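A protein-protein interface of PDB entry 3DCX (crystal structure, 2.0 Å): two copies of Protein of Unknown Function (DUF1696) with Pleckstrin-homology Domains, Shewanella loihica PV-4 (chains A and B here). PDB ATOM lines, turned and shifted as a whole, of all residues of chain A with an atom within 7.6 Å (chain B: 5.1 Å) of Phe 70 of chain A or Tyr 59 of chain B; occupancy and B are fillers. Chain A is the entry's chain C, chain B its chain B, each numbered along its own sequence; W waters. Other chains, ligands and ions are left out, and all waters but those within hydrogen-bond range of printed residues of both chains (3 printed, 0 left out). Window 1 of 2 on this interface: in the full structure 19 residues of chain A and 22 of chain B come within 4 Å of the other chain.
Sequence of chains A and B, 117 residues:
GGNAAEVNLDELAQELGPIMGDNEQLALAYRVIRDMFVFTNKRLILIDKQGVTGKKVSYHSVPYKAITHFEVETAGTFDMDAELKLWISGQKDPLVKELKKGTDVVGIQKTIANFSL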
ATOM      1  N   TYR A  64      -7.309 -27.971  -1.711  1.00  0.00           N
ATOM      2  CA  TYR A  64      -7.944 -26.659  -1.772  1.00  0.00           C
ATOM      3  C   TYR A  64      -7.479 -25.754  -0.638  1.00  0.00           C
ATOM      4  O   TYR A  64      -7.345 -24.528  -0.815  1.00  0.00           O
ATOM      5  CB  TYR A  64      -9.461 -26.799  -1.763  1.00  0.00           C
ATOM      6  CG  TYR A  64     -10.023 -27.334  -3.055  1.00  0.00           C
ATOM      7  CD1 TYR A  64      -9.953 -26.593  -4.223  1.00  0.00           C
ATOM      8  CD2 TYR A  64     -10.641 -28.563  -3.112  1.00  0.00           C
ATOM      9  CE1 TYR A  64     -10.488 -27.063  -5.411  1.00  0.00           C
ATOM     10  CE2 TYR A  64     -11.169 -29.038  -4.304  1.00  0.00           C
ATOM     11  CZ  TYR A  64     -11.084 -28.279  -5.446  1.00  0.00           C
ATOM     12  OH  TYR A  64     -11.590 -28.733  -6.644  1.00  0.00           O
ATOM     13  N   ILE A  67      -4.747 -23.253  -1.397  1.00  0.00           N
ATOM     14  CA  ILE A  67      -5.083 -22.107  -2.207  1.00  0.00           C
ATOM     15  C   ILE A  67      -5.457 -20.949  -1.286  1.00  0.00           C
ATOM     16  O   ILE A  67      -6.548 -20.927  -0.674  1.00  0.00           O
ATOM     17  CB  ILE A  67      -6.243 -22.392  -3.172  1.00  0.00           C
ATOM     18  CG1 ILE A  67      -5.906 -23.535  -4.130  1.00  0.00           C
ATOM     19  CG2 ILE A  67      -6.545 -21.168  -4.001  1.00  0.00           C
ATOM     20  CD1 ILE A  67      -7.072 -23.907  -5.021  1.00  0.00           C
ATOM     21  N   THR A  68      -4.542 -19.992  -1.178  1.00  0.00           N
ATOM     22  CA  THR A  68      -4.655 -18.937  -0.171  1.00  0.00           C
ATOM     23  C   THR A  68      -5.506 -17.764  -0.640  1.00  0.00           C
ATOM     24  O   THR A  68      -6.098 -17.084   0.174  1.00  0.00           O
ATOM     25  CB  THR A  68      -3.280 -18.462   0.267  1.00  0.00           C
ATOM     26  OG1 THR A  68      -2.540 -18.025  -0.873  1.00  0.00           O
ATOM     27  CG2 THR A  68      -2.530 -19.588   0.951  1.00  0.00           C
ATOM     28  N   HIS A  69      -5.521 -17.520  -1.947  1.00  0.00           N
ATOM     29  CA  HIS A  69      -6.364 -16.551  -2.570  1.00  0.00           C
ATOM     30  C   HIS A  69      -6.391 -16.854  -4.067  1.00  0.00           C
ATOM     31  O   HIS A  69      -5.579 -17.631  -4.567  1.00  0.00           O
ATOM     32  CB  HIS A  69      -5.993 -15.088  -2.210  1.00  0.00           C
ATOM     33  CG  HIS A  69      -4.612 -14.631  -2.613  1.00  0.00           C
ATOM     34  ND1 HIS A  69      -4.413 -13.486  -3.345  1.00  0.00           N
ATOM     35  CD2 HIS A  69      -3.372 -15.086  -2.295  1.00  0.00           C
ATOM     36  CE1 HIS A  69      -3.116 -13.286  -3.523  1.00  0.00           C
ATOM     37  NE2 HIS A  69      -2.457 -14.252  -2.903  1.00  0.00           N
ATOM     38  N   PHE A  70      -7.370 -16.304  -4.765  1.00  0.00           N
ATOM     39  CA  PHE A  70      -7.529 -16.572  -6.196  1.00  0.00           C
ATOM     40  C   PHE A  70      -8.286 -15.440  -6.877  1.00  0.00           C
ATOM     41  O   PHE A  70      -8.988 -14.651  -6.224  1.00  0.00           O
ATOM     42  CB  PHE A  70      -8.244 -17.907  -6.456  1.00  0.00           C
ATOM     43  CG  PHE A  70      -9.602 -18.020  -5.814  1.00  0.00           C
ATOM     44  CD1 PHE A  70      -9.737 -18.451  -4.505  1.00  0.00           C
ATOM     45  CD2 PHE A  70     -10.743 -17.690  -6.520  1.00  0.00           C
ATOM     46  CE1 PHE A  70     -10.969 -18.544  -3.917  1.00  0.00           C
ATOM     47  CE2 PHE A  70     -11.959 -17.796  -5.942  1.00  0.00           C
ATOM     48  CZ  PHE A  70     -12.083 -18.242  -4.649  1.00  0.00           C
ATOM     49  N   GLU A  71      -8.122 -15.365  -8.194  1.00  0.00           N
ATOM     50  CA  GLU A  71      -8.608 -14.217  -8.935  1.00  0.00           C
ATOM     51  C   GLU A  71      -9.045 -14.628 -10.314  1.00  0.00           C
ATOM     52  O   GLU A  71      -8.368 -15.391 -10.963  1.00  0.00           O
ATOM     53  CB  GLU A  71      -7.483 -13.157  -9.018  1.00  0.00           C
ATOM     54  CG  GLU A  71      -7.907 -11.858  -9.698  1.00  0.00           C
ATOM     55  CD  GLU A  71      -6.724 -10.915  -9.975  1.00  0.00           C
ATOM     56  OE1 GLU A  71      -5.590 -11.206  -9.547  1.00  0.00           O
ATOM     57  OE2 GLU A  71      -6.928  -9.890 -10.630  1.00  0.00           O
ATOM     58  N   VAL A  72     -10.180 -14.115 -10.777  1.00  0.00           N
ATOM     59  CA  VAL A  72     -10.526 -14.241 -12.186  1.00  0.00           C
ATOM     60  C   VAL A  72     -10.611 -12.825 -12.767  1.00  0.00           C
ATOM     61  O   VAL A  72     -11.330 -11.942 -12.224  1.00  0.00           O
ATOM     62  CB  VAL A  72     -11.827 -15.031 -12.384  1.00  0.00           C
ATOM     63  CG1 VAL A  72     -12.223 -15.059 -13.832  1.00  0.00           C
ATOM     64  CG2 VAL A  72     -11.653 -16.445 -11.860  1.00  0.00           C
ATOM     65  N   GLU A  73      -9.846 -12.605 -13.843  1.00  0.00           N
ATOM     66  CA  GLU A  73      -9.865 -11.351 -14.590  1.00  0.00           C
ATOM     67  C   GLU A  73     -10.326 -11.606 -16.009  1.00  0.00           C
ATOM     68  O   GLU A  73      -9.842 -12.531 -16.639  1.00  0.00           O
ATOM     69  CB  GLU A  73      -8.464 -10.775 -14.633  1.00  0.00           C
ATOM     70  CG  GLU A  73      -8.380  -9.418 -15.270  1.00  0.00           C
ATOM     71  CD  GLU A  73      -7.034  -8.790 -15.035  1.00  0.00           C
ATOM     72  OE1 GLU A  73      -6.022  -9.508 -15.185  1.00  0.00           O
ATOM     73  OE2 GLU A  73      -7.002  -7.592 -14.673  1.00  0.00           O
ATOM     74  N   THR A  74     -11.258 -10.791 -16.498  1.00  0.00           N
ATOM     75  CA  THR A  74     -11.796 -10.899 -17.862  1.00  0.00           C
ATOM     76  C   THR A  74     -11.425  -9.689 -18.716  1.00  0.00           C
ATOM     77  O   THR A  74     -11.491  -8.555 -18.237  1.00  0.00           O
ATOM     78  CB  THR A  74     -13.341 -10.966 -17.821  1.00  0.00           C
ATOM     79  OG1 THR A  74     -13.747 -11.987 -16.888  1.00  0.00           O
ATOM     80  CG2 THR A  74     -13.941 -11.250 -19.247  1.00  0.00           C
ATOM     81  N   GLU A  83      -8.592 -15.052 -17.354  1.00  0.00           N
ATOM     82  CA  GLU A  83      -7.447 -15.703 -16.715  1.00  0.00           C
ATOM     83  C   GLU A  83      -7.832 -16.012 -15.299  1.00  0.00           C
ATOM     84  O   GLU A  83      -8.355 -15.141 -14.582  1.00  0.00           O
ATOM     85  CB  GLU A  83      -6.193 -14.801 -16.698  1.00  0.00           C
ATOM     86  CG  GLU A  83      -5.384 -14.810 -17.985  1.00  0.00           C
ATOM     87  CD  GLU A  83      -4.001 -14.123 -17.846  1.00  0.00           C
ATOM     88  OE1 GLU A  83      -3.730 -13.460 -16.813  1.00  0.00           O
ATOM     89  OE2 GLU A  83      -3.193 -14.273 -18.791  1.00  0.00           O
ATOM     90  N   LEU A  84      -7.583 -17.249 -14.898  1.00  0.00           N
ATOM     91  CA  LEU A  84      -7.680 -17.656 -13.479  1.00  0.00           C
ATOM     92  C   LEU A  84      -6.288 -17.617 -12.878  1.00  0.00           C
ATOM     93  O   LEU A  84      -5.355 -18.145 -13.461  1.00  0.00           O
ATOM     94  CB  LEU A  84      -8.242 -19.068 -13.368  1.00  0.00           C
ATOM     95  CG  LEU A  84      -8.250 -19.719 -11.986  1.00  0.00           C
ATOM     96  CD1 LEU A  84      -9.185 -19.000 -11.047  1.00  0.00           C
ATOM     97  CD2 LEU A  84      -8.656 -21.179 -12.102  1.00  0.00           C
ATOM     98  N   LYS A  85      -6.140 -16.958 -11.726  1.00  0.00           N
ATOM     99  CA  LYS A  85      -4.905 -16.984 -10.969  1.00  0.00           C
ATOM    100  C   LYS A  85      -5.201 -17.663  -9.645  1.00  0.00           C
ATOM    101  O   LYS A  85      -6.195 -17.351  -8.973  1.00  0.00           O
ATOM    102  CB  LYS A  85      -4.340 -15.588 -10.721  1.00  0.00           C
ATOM    103  CG  LYS A  85      -3.887 -14.858 -11.994  1.00  0.00           C
ATOM    104  CD  LYS A  85      -3.179 -13.512 -11.698  1.00  0.00           C
ATOM    105  CE  LYS A  85      -2.591 -12.891 -12.977  1.00  0.00           C
ATOM    106  NZ  LYS A  85      -2.384 -11.409 -12.892  1.00  0.00           N
ATOM    107  N   LEU A  86      -4.330 -18.602  -9.292  1.00  0.00           N
ATOM    108  CA  LEU A  86      -4.429 -19.352  -8.056  1.00  0.00           C
ATOM    109  C   LEU A  86      -3.113 -19.186  -7.307  1.00  0.00           C
ATOM    110  O   LEU A  86      -2.046 -19.533  -7.821  1.00  0.00           O
ATOM    111  CB  LEU A  86      -4.689 -20.839  -8.361  1.00  0.00           C
ATOM    112  CG  LEU A  86      -6.014 -21.208  -9.037  1.00  0.00           C
ATOM    113  CD1 LEU A  86      -5.919 -22.593  -9.671  1.00  0.00           C
ATOM    114  CD2 LEU A  86      -7.161 -21.168  -8.047  1.00  0.00           C
ATOM    115  N   TRP A  87      -3.175 -18.640  -6.095  1.00  0.00           N
ATOM    116  CA  TRP A  87      -2.009 -18.570  -5.259  1.00  0.00           C
ATOM    117  C   TRP A  87      -1.964 -19.770  -4.338  1.00  0.00           C
ATOM    118  O   TRP A  87      -2.936 -20.052  -3.626  1.00  0.00           O
ATOM    119  CB  TRP A  87      -1.971 -17.261  -4.464  1.00  0.00           C
ATOM    120  CG  TRP A  87      -1.556 -16.075  -5.276  1.00  0.00           C
ATOM    121  CD1 TRP A  87      -0.302 -15.538  -5.376  1.00  0.00           C
ATOM    122  CD2 TRP A  87      -2.409 -15.240  -6.033  1.00  0.00           C
ATOM    123  NE1 TRP A  87      -0.319 -14.438  -6.198  1.00  0.00           N
ATOM    124  CE2 TRP A  87      -1.607 -14.228  -6.606  1.00  0.00           C
ATOM    125  CE3 TRP A  87      -3.781 -15.270  -6.337  1.00  0.00           C
ATOM    126  CZ2 TRP A  87      -2.134 -13.251  -7.433  1.00  0.00           C
ATOM    127  CZ3 TRP A  87      -4.298 -14.293  -7.136  1.00  0.00           C
ATOM    128  CH2 TRP A  87      -3.482 -13.310  -7.694  1.00  0.00           C
ATOM    129  N   PRO A  94       1.686 -16.935  -8.757  1.00  0.00           N
ATOM    130  CA  PRO A  94       0.470 -17.673  -8.907  1.00  0.00           C
ATOM    131  C   PRO A  94       0.503 -18.582 -10.110  1.00  0.00           C
ATOM    132  O   PRO A  94       1.210 -18.338 -11.073  1.00  0.00           O
ATOM    133  CB  PRO A  94      -0.570 -16.583  -9.110  1.00  0.00           C
ATOM    134  CG  PRO A  94       0.159 -15.523  -9.797  1.00  0.00           C
ATOM    135  CD  PRO A  94       1.495 -15.520  -9.125  1.00  0.00           C
ATOM    136  N   ILE A 108     -16.231 -23.024 -13.045  1.00  0.00           N
ATOM    137  CA  ILE A 108     -14.914 -23.093 -12.427  1.00  0.00           C
ATOM    138  C   ILE A 108     -14.908 -22.272 -11.137  1.00  0.00           C
ATOM    139  O   ILE A 108     -14.456 -22.735 -10.075  1.00  0.00           O
ATOM    140  CB  ILE A 108     -13.814 -22.588 -13.414  1.00  0.00           C
ATOM    141  CG1 ILE A 108     -13.583 -23.619 -14.524  1.00  0.00           C
ATOM    142  CG2 ILE A 108     -12.491 -22.252 -12.678  1.00  0.00           C
ATOM    143  CD1 ILE A 108     -12.937 -23.089 -15.716  1.00  0.00           C
ATOM    144  N   GLN A 109     -15.456 -21.068 -11.226  1.00  0.00           N
ATOM    145  CA  GLN A 109     -15.514 -20.185 -10.080  1.00  0.00           C
ATOM    146  C   GLN A 109     -16.424 -20.757  -9.003  1.00  0.00           C
ATOM    147  O   GLN A 109     -16.074 -20.721  -7.820  1.00  0.00           O
ATOM    148  CB  GLN A 109     -15.968 -18.803 -10.505  1.00  0.00           C
ATOM    149  CG  GLN A 109     -14.919 -18.054 -11.268  1.00  0.00           C
ATOM    150  CD  GLN A 109     -15.445 -16.721 -11.802  1.00  0.00           C
ATOM    151  OE1 GLN A 109     -15.960 -16.652 -12.926  1.00  0.00           O
ATOM    152  NE2 GLN A 109     -15.278 -15.662 -11.012  1.00  0.00           N
ATOM    153  N   LYS A 110     -17.550 -21.326  -9.416  1.00  0.00           N
ATOM    154  CA  LYS A 110     -18.505 -21.965  -8.491  1.00  0.00           C
ATOM    155  C   LYS A 110     -17.855 -23.148  -7.738  1.00  0.00           C
ATOM    156  O   LYS A 110     -17.982 -23.284  -6.511  1.00  0.00           O
ATOM    157  CB  LYS A 110     -19.700 -22.460  -9.287  1.00  0.00           C
ATOM    158  CG  LYS A 110     -20.744 -23.185  -8.471  1.00  0.00           C
ATOM    159  CD  LYS A 110     -21.575 -22.236  -7.687  1.00  0.00           C
ATOM    160  CE  LYS A 110     -22.557 -22.995  -6.866  1.00  0.00           C
ATOM    161  NZ  LYS A 110     -23.255 -22.158  -5.902  1.00  0.00           N
ATOM    162  N   ILE A 112     -14.523 -23.767  -7.301  1.00  0.00           N
ATOM    163  CA  ILE A 112     -13.542 -23.265  -6.351  1.00  0.00           C
ATOM    164  C   ILE A 112     -14.215 -22.726  -5.085  1.00  0.00           C
ATOM    165  O   ILE A 112     -13.795 -23.045  -3.982  1.00  0.00           O
ATOM    166  CB  ILE A 112     -12.597 -22.205  -6.981  1.00  0.00           C
ATOM    167  CG1 ILE A 112     -11.673 -22.862  -7.996  1.00  0.00           C
ATOM    168  CG2 ILE A 112     -11.699 -21.511  -5.898  1.00  0.00           C
ATOM    169  CD1 ILE A 112     -11.142 -21.885  -9.035  1.00  0.00           C
ATOM    170  N   ALA A 113     -15.272 -21.953  -5.229  1.00  0.00           N
ATOM    171  CA  ALA A 113     -15.976 -21.442  -4.047  1.00  0.00           C
ATOM    172  C   ALA A 113     -16.556 -22.573  -3.170  1.00  0.00           C
ATOM    173  O   ALA A 113     -16.424 -22.562  -1.945  1.00  0.00           O
ATOM    174  CB  ALA A 113     -17.087 -20.472  -4.468  1.00  0.00           C
ATOM    175  N   ASN A 114     -17.211 -23.535  -3.813  1.00  0.00           N
ATOM    176  CA  ASN A 114     -17.762 -24.680  -3.107  1.00  0.00           C
ATOM    177  C   ASN A 114     -16.733 -25.491  -2.336  1.00  0.00           C
ATOM    178  O   ASN A 114     -16.994 -25.918  -1.242  1.00  0.00           O
ATOM    179  CB  ASN A 114     -18.522 -25.614  -4.049  1.00  0.00           C
ATOM    180  CG  ASN A 114     -19.991 -25.310  -4.103  1.00  0.00           C
ATOM    181  OD1 ASN A 114     -20.514 -24.542  -3.296  1.00  0.00           O
ATOM    182  ND2 ASN A 114     -20.674 -25.898  -5.063  1.00  0.00           N
ATOM    183  N   SER A 116     -13.190 -24.691  -1.793  1.00  0.00           N
ATOM    184  CA  SER A 116     -12.049 -24.044  -1.143  1.00  0.00           C
ATOM    185  C   SER A 116     -12.437 -23.169   0.051  1.00  0.00           C
ATOM    186  O   SER A 116     -11.607 -22.881   0.898  1.00  0.00           O
ATOM    187  CB  SER A 116     -11.271 -23.191  -2.147  1.00  0.00           C
ATOM    188  OG  SER A 116     -11.922 -21.946  -2.356  1.00  0.00           O
ATOM    189  N   LEU A 117     -13.685 -22.744   0.121  1.00  0.00           N
ATOM    190  CA  LEU A 117     -14.036 -21.732   1.094  1.00  0.00           C
ATOM    191  C   LEU A 117     -14.608 -22.311   2.388  1.00  0.00           C
ATOM    192  O   LEU A 117     -15.313 -23.332   2.409  1.00  0.00           O
ATOM    193  CB  LEU A 117     -15.005 -20.714   0.478  1.00  0.00           C
ATOM    194  CG  LEU A 117     -14.504 -19.902  -0.719  1.00  0.00           C
ATOM    195  CD1 LEU A 117     -15.679 -19.046  -1.218  1.00  0.00           C
ATOM    196  CD2 LEU A 117     -13.292 -19.067  -0.384  1.00  0.00           C
ATOM    197  OXT LEU A 117     -14.371 -21.714   3.442  1.00  0.00           O
ATOM    198  N   LEU B  16     -23.994 -11.851  -7.971  1.00  0.00           N
ATOM    199  CA  LEU B  16     -22.852 -12.677  -7.614  1.00  0.00           C
ATOM    200  C   LEU B  16     -23.158 -14.172  -7.433  1.00  0.00           C
ATOM    201  O   LEU B  16     -22.241 -14.993  -7.515  1.00  0.00           O
ATOM    202  CB  LEU B  16     -22.186 -12.166  -6.334  1.00  0.00           C
ATOM    203  CG  LEU B  16     -21.588 -10.752  -6.452  1.00  0.00           C
ATOM    204  CD1 LEU B  16     -20.878 -10.370  -5.155  1.00  0.00           C
ATOM    205  CD2 LEU B  16     -20.663 -10.656  -7.666  1.00  0.00           C
ATOM    206  N   ILE B  19     -21.231 -17.241  -8.908  1.00  0.00           N
ATOM    207  CA  ILE B  19     -19.845 -17.535  -8.528  1.00  0.00           C
ATOM    208  C   ILE B  19     -19.637 -17.718  -7.008  1.00  0.00           C
ATOM    209  O   ILE B  19     -18.494 -17.839  -6.551  1.00  0.00           O
ATOM    210  CB  ILE B  19     -18.857 -16.486  -9.114  1.00  0.00           C
ATOM    211  CG1 ILE B  19     -19.101 -15.119  -8.484  1.00  0.00           C
ATOM    212  CG2 ILE B  19     -19.000 -16.436 -10.666  1.00  0.00           C
ATOM    213  CD1 ILE B  19     -17.981 -14.139  -8.639  1.00  0.00           C
ATOM    214  N   ARG B  43     -15.304 -14.820   2.532  1.00  0.00           N
ATOM    215  CA  ARG B  43     -14.183 -14.144   1.885  1.00  0.00           C
ATOM    216  C   ARG B  43     -14.498 -12.701   1.613  1.00  0.00           C
ATOM    217  O   ARG B  43     -15.670 -12.306   1.547  1.00  0.00           O
ATOM    218  CB  ARG B  43     -13.838 -14.847   0.530  1.00  0.00           C
ATOM    219  CG  ARG B  43     -15.060 -15.024  -0.331  1.00  0.00           C
ATOM    220  CD  ARG B  43     -14.804 -15.435  -1.764  1.00  0.00           C
ATOM    221  NE  ARG B  43     -16.043 -15.956  -2.321  1.00  0.00           N
ATOM    222  CZ  ARG B  43     -16.216 -16.365  -3.577  1.00  0.00           C
ATOM    223  NH1 ARG B  43     -15.256 -16.258  -4.471  1.00  0.00           N
ATOM    224  NH2 ARG B  43     -17.384 -16.850  -3.941  1.00  0.00           N
ATOM    225  N   ILE B  45     -14.250 -10.274  -1.483  1.00  0.00           N
ATOM    226  CA  ILE B  45     -14.061 -10.180  -2.925  1.00  0.00           C
ATOM    227  C   ILE B  45     -13.815  -8.722  -3.298  1.00  0.00           C
ATOM    228  O   ILE B  45     -14.649  -7.840  -3.041  1.00  0.00           O
ATOM    229  CB  ILE B  45     -15.300 -10.740  -3.717  1.00  0.00           C
ATOM    230  CG1 ILE B  45     -15.702 -12.139  -3.204  1.00  0.00           C
ATOM    231  CG2 ILE B  45     -15.024 -10.742  -5.257  1.00  0.00           C
ATOM    232  CD1 ILE B  45     -17.156 -12.554  -3.611  1.00  0.00           C
ATOM    233  N   LEU B  46     -12.649  -8.464  -3.875  1.00  0.00           N
ATOM    234  CA  LEU B  46     -12.315  -7.153  -4.415  1.00  0.00           C
ATOM    235  C   LEU B  46     -12.692  -7.154  -5.891  1.00  0.00           C
ATOM    236  O   LEU B  46     -12.104  -7.918  -6.683  1.00  0.00           O
ATOM    237  CB  LEU B  46     -10.822  -6.878  -4.290  1.00  0.00           C
ATOM    238  CG  LEU B  46     -10.185  -6.940  -2.909  1.00  0.00           C
ATOM    239  CD1 LEU B  46      -8.723  -6.548  -3.031  1.00  0.00           C
ATOM    240  CD2 LEU B  46     -10.905  -6.029  -1.944  1.00  0.00           C
ATOM    241  N   ILE B  47     -13.672  -6.320  -6.259  1.00  0.00           N
ATOM    242  CA  ILE B  47     -14.110  -6.206  -7.656  1.00  0.00           C
ATOM    243  C   ILE B  47     -13.534  -4.919  -8.204  1.00  0.00           C
ATOM    244  O   ILE B  47     -13.901  -3.847  -7.767  1.00  0.00           O
ATOM    245  CB  ILE B  47     -15.662  -6.236  -7.812  1.00  0.00           C
ATOM    246  CG1 ILE B  47     -16.264  -7.435  -7.077  1.00  0.00           C
ATOM    247  CG2 ILE B  47     -16.076  -6.267  -9.303  1.00  0.00           C
ATOM    248  CD1 ILE B  47     -17.807  -7.482  -7.124  1.00  0.00           C
ATOM    249  N   VAL B  57     -12.368  -6.407 -15.886  1.00  0.00           N
ATOM    250  CA  VAL B  57     -12.852  -6.563 -14.529  1.00  0.00           C
ATOM    251  C   VAL B  57     -12.148  -7.741 -13.875  1.00  0.00           C
ATOM    252  O   VAL B  57     -12.018  -8.798 -14.486  1.00  0.00           O
ATOM    253  CB  VAL B  57     -14.363  -6.847 -14.495  1.00  0.00           C
ATOM    254  CG1 VAL B  57     -14.848  -7.002 -13.053  1.00  0.00           C
ATOM    255  CG2 VAL B  57     -15.139  -5.754 -15.183  1.00  0.00           C
ATOM    256  N   SER B  58     -11.714  -7.546 -12.633  1.00  0.00           N
ATOM    257  CA  SER B  58     -11.178  -8.641 -11.838  1.00  0.00           C
ATOM    258  C   SER B  58     -11.980  -8.825 -10.559  1.00  0.00           C
ATOM    259  O   SER B  58     -12.420  -7.843  -9.921  1.00  0.00           O
ATOM    260  CB  SER B  58      -9.685  -8.448 -11.531  1.00  0.00           C
ATOM    261  OG  SER B  58      -9.408  -7.130 -11.118  1.00  0.00           O
ATOM    262  N   TYR B  59     -12.211 -10.102 -10.230  1.00  0.00           N
ATOM    263  CA  TYR B  59     -12.784 -10.551  -8.973  1.00  0.00           C
ATOM    264  C   TYR B  59     -11.692 -11.311  -8.205  1.00  0.00           C
ATOM    265  O   TYR B  59     -11.374 -12.459  -8.542  1.00  0.00           O
ATOM    266  CB  TYR B  59     -13.989 -11.509  -9.190  1.00  0.00           C
ATOM    267  CG  TYR B  59     -15.184 -10.896  -9.876  1.00  0.00           C
ATOM    268  CD1 TYR B  59     -15.155 -10.611 -11.227  1.00  0.00           C
ATOM    269  CD2 TYR B  59     -16.334 -10.600  -9.185  1.00  0.00           C
ATOM    270  CE1 TYR B  59     -16.238 -10.048 -11.851  1.00  0.00           C
ATOM    271  CE2 TYR B  59     -17.426 -10.029  -9.811  1.00  0.00           C
ATOM    272  CZ  TYR B  59     -17.368  -9.757 -11.143  1.00  0.00           C
ATOM    273  OH  TYR B  59     -18.446  -9.202 -11.798  1.00  0.00           O
ATOM    274  N   HIS B  60     -11.167 -10.695  -7.144  1.00  0.00           N
ATOM    275  CA  HIS B  60     -10.054 -11.230  -6.379  1.00  0.00           C
ATOM    276  C   HIS B  60     -10.614 -11.619  -5.026  1.00  0.00           C
ATOM    277  O   HIS B  60     -11.075 -10.770  -4.275  1.00  0.00           O
ATOM    278  CB  HIS B  60      -8.931 -10.193  -6.226  1.00  0.00           C
ATOM    279  CG  HIS B  60      -7.645 -10.744  -5.668  1.00  0.00           C
ATOM    280  ND1 HIS B  60      -6.411 -10.204  -5.966  1.00  0.00           N
ATOM    281  CD2 HIS B  60      -7.403 -11.779  -4.832  1.00  0.00           C
ATOM    282  CE1 HIS B  60      -5.469 -10.895  -5.347  1.00  0.00           C
ATOM    283  NE2 HIS B  60      -6.044 -11.862  -4.659  1.00  0.00           N
ATOM    284  N   SER B  61     -10.602 -12.914  -4.758  1.00  0.00           N
ATOM    285  CA  SER B  61     -11.127 -13.491  -3.502  1.00  0.00           C
ATOM    286  C   SER B  61     -10.024 -13.762  -2.480  1.00  0.00           C
ATOM    287  O   SER B  61      -9.038 -14.451  -2.758  1.00  0.00           O
ATOM    288  CB  SER B  61     -11.896 -14.770  -3.795  1.00  0.00           C
ATOM    289  OG  SER B  61     -13.049 -14.539  -4.606  1.00  0.00           O
ATOM    290  N   PRO B  63     -10.064 -15.362   1.189  1.00  0.00           N
ATOM    291  CA  PRO B  63     -10.767 -16.036   2.289  1.00  0.00           C
ATOM    292  C   PRO B  63     -10.245 -15.497   3.602  1.00  0.00           C
ATOM    293  O   PRO B  63      -9.026 -15.301   3.753  1.00  0.00           O
ATOM    294  CB  PRO B  63     -10.375 -17.511   2.123  1.00  0.00           C
ATOM    295  CG  PRO B  63      -9.869 -17.629   0.782  1.00  0.00           C
ATOM    296  CD  PRO B  63      -9.348 -16.321   0.353  1.00  0.00           C
HETATM  297  O   HOH W   1     -15.869 -17.977  -6.955  1.00  0.00           O
HETATM  298  O   HOH W   2      -9.068  -5.319 -13.276  1.00  0.00           O
HETATM  299  O   HOH W   3     -14.226 -11.253 -14.444  1.00  0.00           O
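Pro 63 of chain B touches Thr 68 of chain A. CB of His 69 of chain A touches O of Ser 61 of chain B, 3.2 Å away. His 60 of chain B touches Phe 70 of chain A (CD2 to O, 3.6 Å). Ser 58 of chain B touches Glu 71 of chain A (CB to OE2, 3.2 Å). Glu 71 of chain A touches His 60 of chain B. CA of Glu 73 of chain A touches O of Val 57 of chain B, 3.3 Å away. Trp 87 of chain A touches His 60 of chain B (CZ3 to NE2, 3.9 Å). CB of Ala 113 of chain A touches O of Ile 19 of chain B (3.6 Å). Leu 117 of chain A touches Arg 43 of chain B. Leu 117 of chain A touches Pro 63 of chain B.
Of the printed residues of chain B, Phe 70 of chain A touches Arg 43, Tyr 59, His 60 and Ser 61. Printed residues of chain B within 4 Å of Leu 117 of chain A: Arg 43 (3.3 Å) and Pro 63 (3.9 Å). Printed residues of chain B within 4 Å of Glu 73 of chain A: Val 57 (3.3 Å). Of the printed residues of chain B, Thr 74 of chain A touches Val 57. Lys 110 of chain A touches none of the printed residues of chain B. The nearest printed residue of chain B that does not touch Phe 70 of chain A is Pro 63 of chain B (4.9 Å). The nearest printed residue of chain A that does not touch Tyr 59 of chain B is Gln 109 of chain A (4.7 Å). The nearest printed residue of chain A that does not touch His 60 of chain B is Val 72 of chain A (5.1 Å).
The backbone carbonyl oxygen (O) of His 69 of chain A lies within hydrogen-bond range of the backbone NH (N) of Trp 87 of chain A (3.0 Å). The backbone carbonyl oxygen (O) of His 60 of chain B lies within hydrogen-bond range of the backbone NH (N) of Leu 46 of chain B, at 2.8 Å. O of Ile 19 of chain B sits at hydrogen-bond distance from NH2 of Arg 43 of chain B (3.0 Å). The backbone carbonyl oxygen (O) of Glu 73 of chain A is in hydrogen-bond range of the backbone NH (N) of Glu 83 of chain A. N of Thr 68 of chain A is in hydrogen-bond range of O of Trp 87 of chain A, 2.9 Å away. NH1 of Arg 43 of chain B lies within hydrogen-bond range of OG of Ser 61 of chain B (2.8 Å).
Water W3 bridges the side-chain hydroxyl of Thr 74 of chain A and the backbone carbonyl oxygen of Val 57 of chain B. Water W1 lies within hydrogen-bond range of the backbone carbonyl oxygen of Ile 19 of chain B, the backbone carbonyl oxygen of Gln 109 of chain A and the guanidinium group of Arg 43 of chain B. Water W2 bridges the side-chain hydroxyl (OG) of Ser 58 of chain B (2.8 Å) and the side-chain carboxylate (OE2) of Glu 73 of chain A (3.4 Å).
Of the 23 printed residues of chain A, 11 touch a printed residue of chain B. Along chain B the printed residues that touch a printed residue of chain A span positions 19 to 63. Among the printed residues, 21 pairs touch across the chains.
No position is printed for both chains.
A ring nitrogen (NE2) of His 60 of chain B sits at hydrogen-bond distance from a ring nitrogen (ND1) of His 69 of chain A. The backbone NH (N) of Tyr 59 of chain B lies within hydrogen-bond range of the backbone carbonyl oxygen (O) of Val 72 of chain A (2.9 Å). O of Phe 70 of chain A is in hydrogen-bond range of N of Ser 61 of chain B, 2.8 Å away. N of Thr 74 of chain A sits at hydrogen-bond distance from O of Val 57 of chain B, at 2.9 Å.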
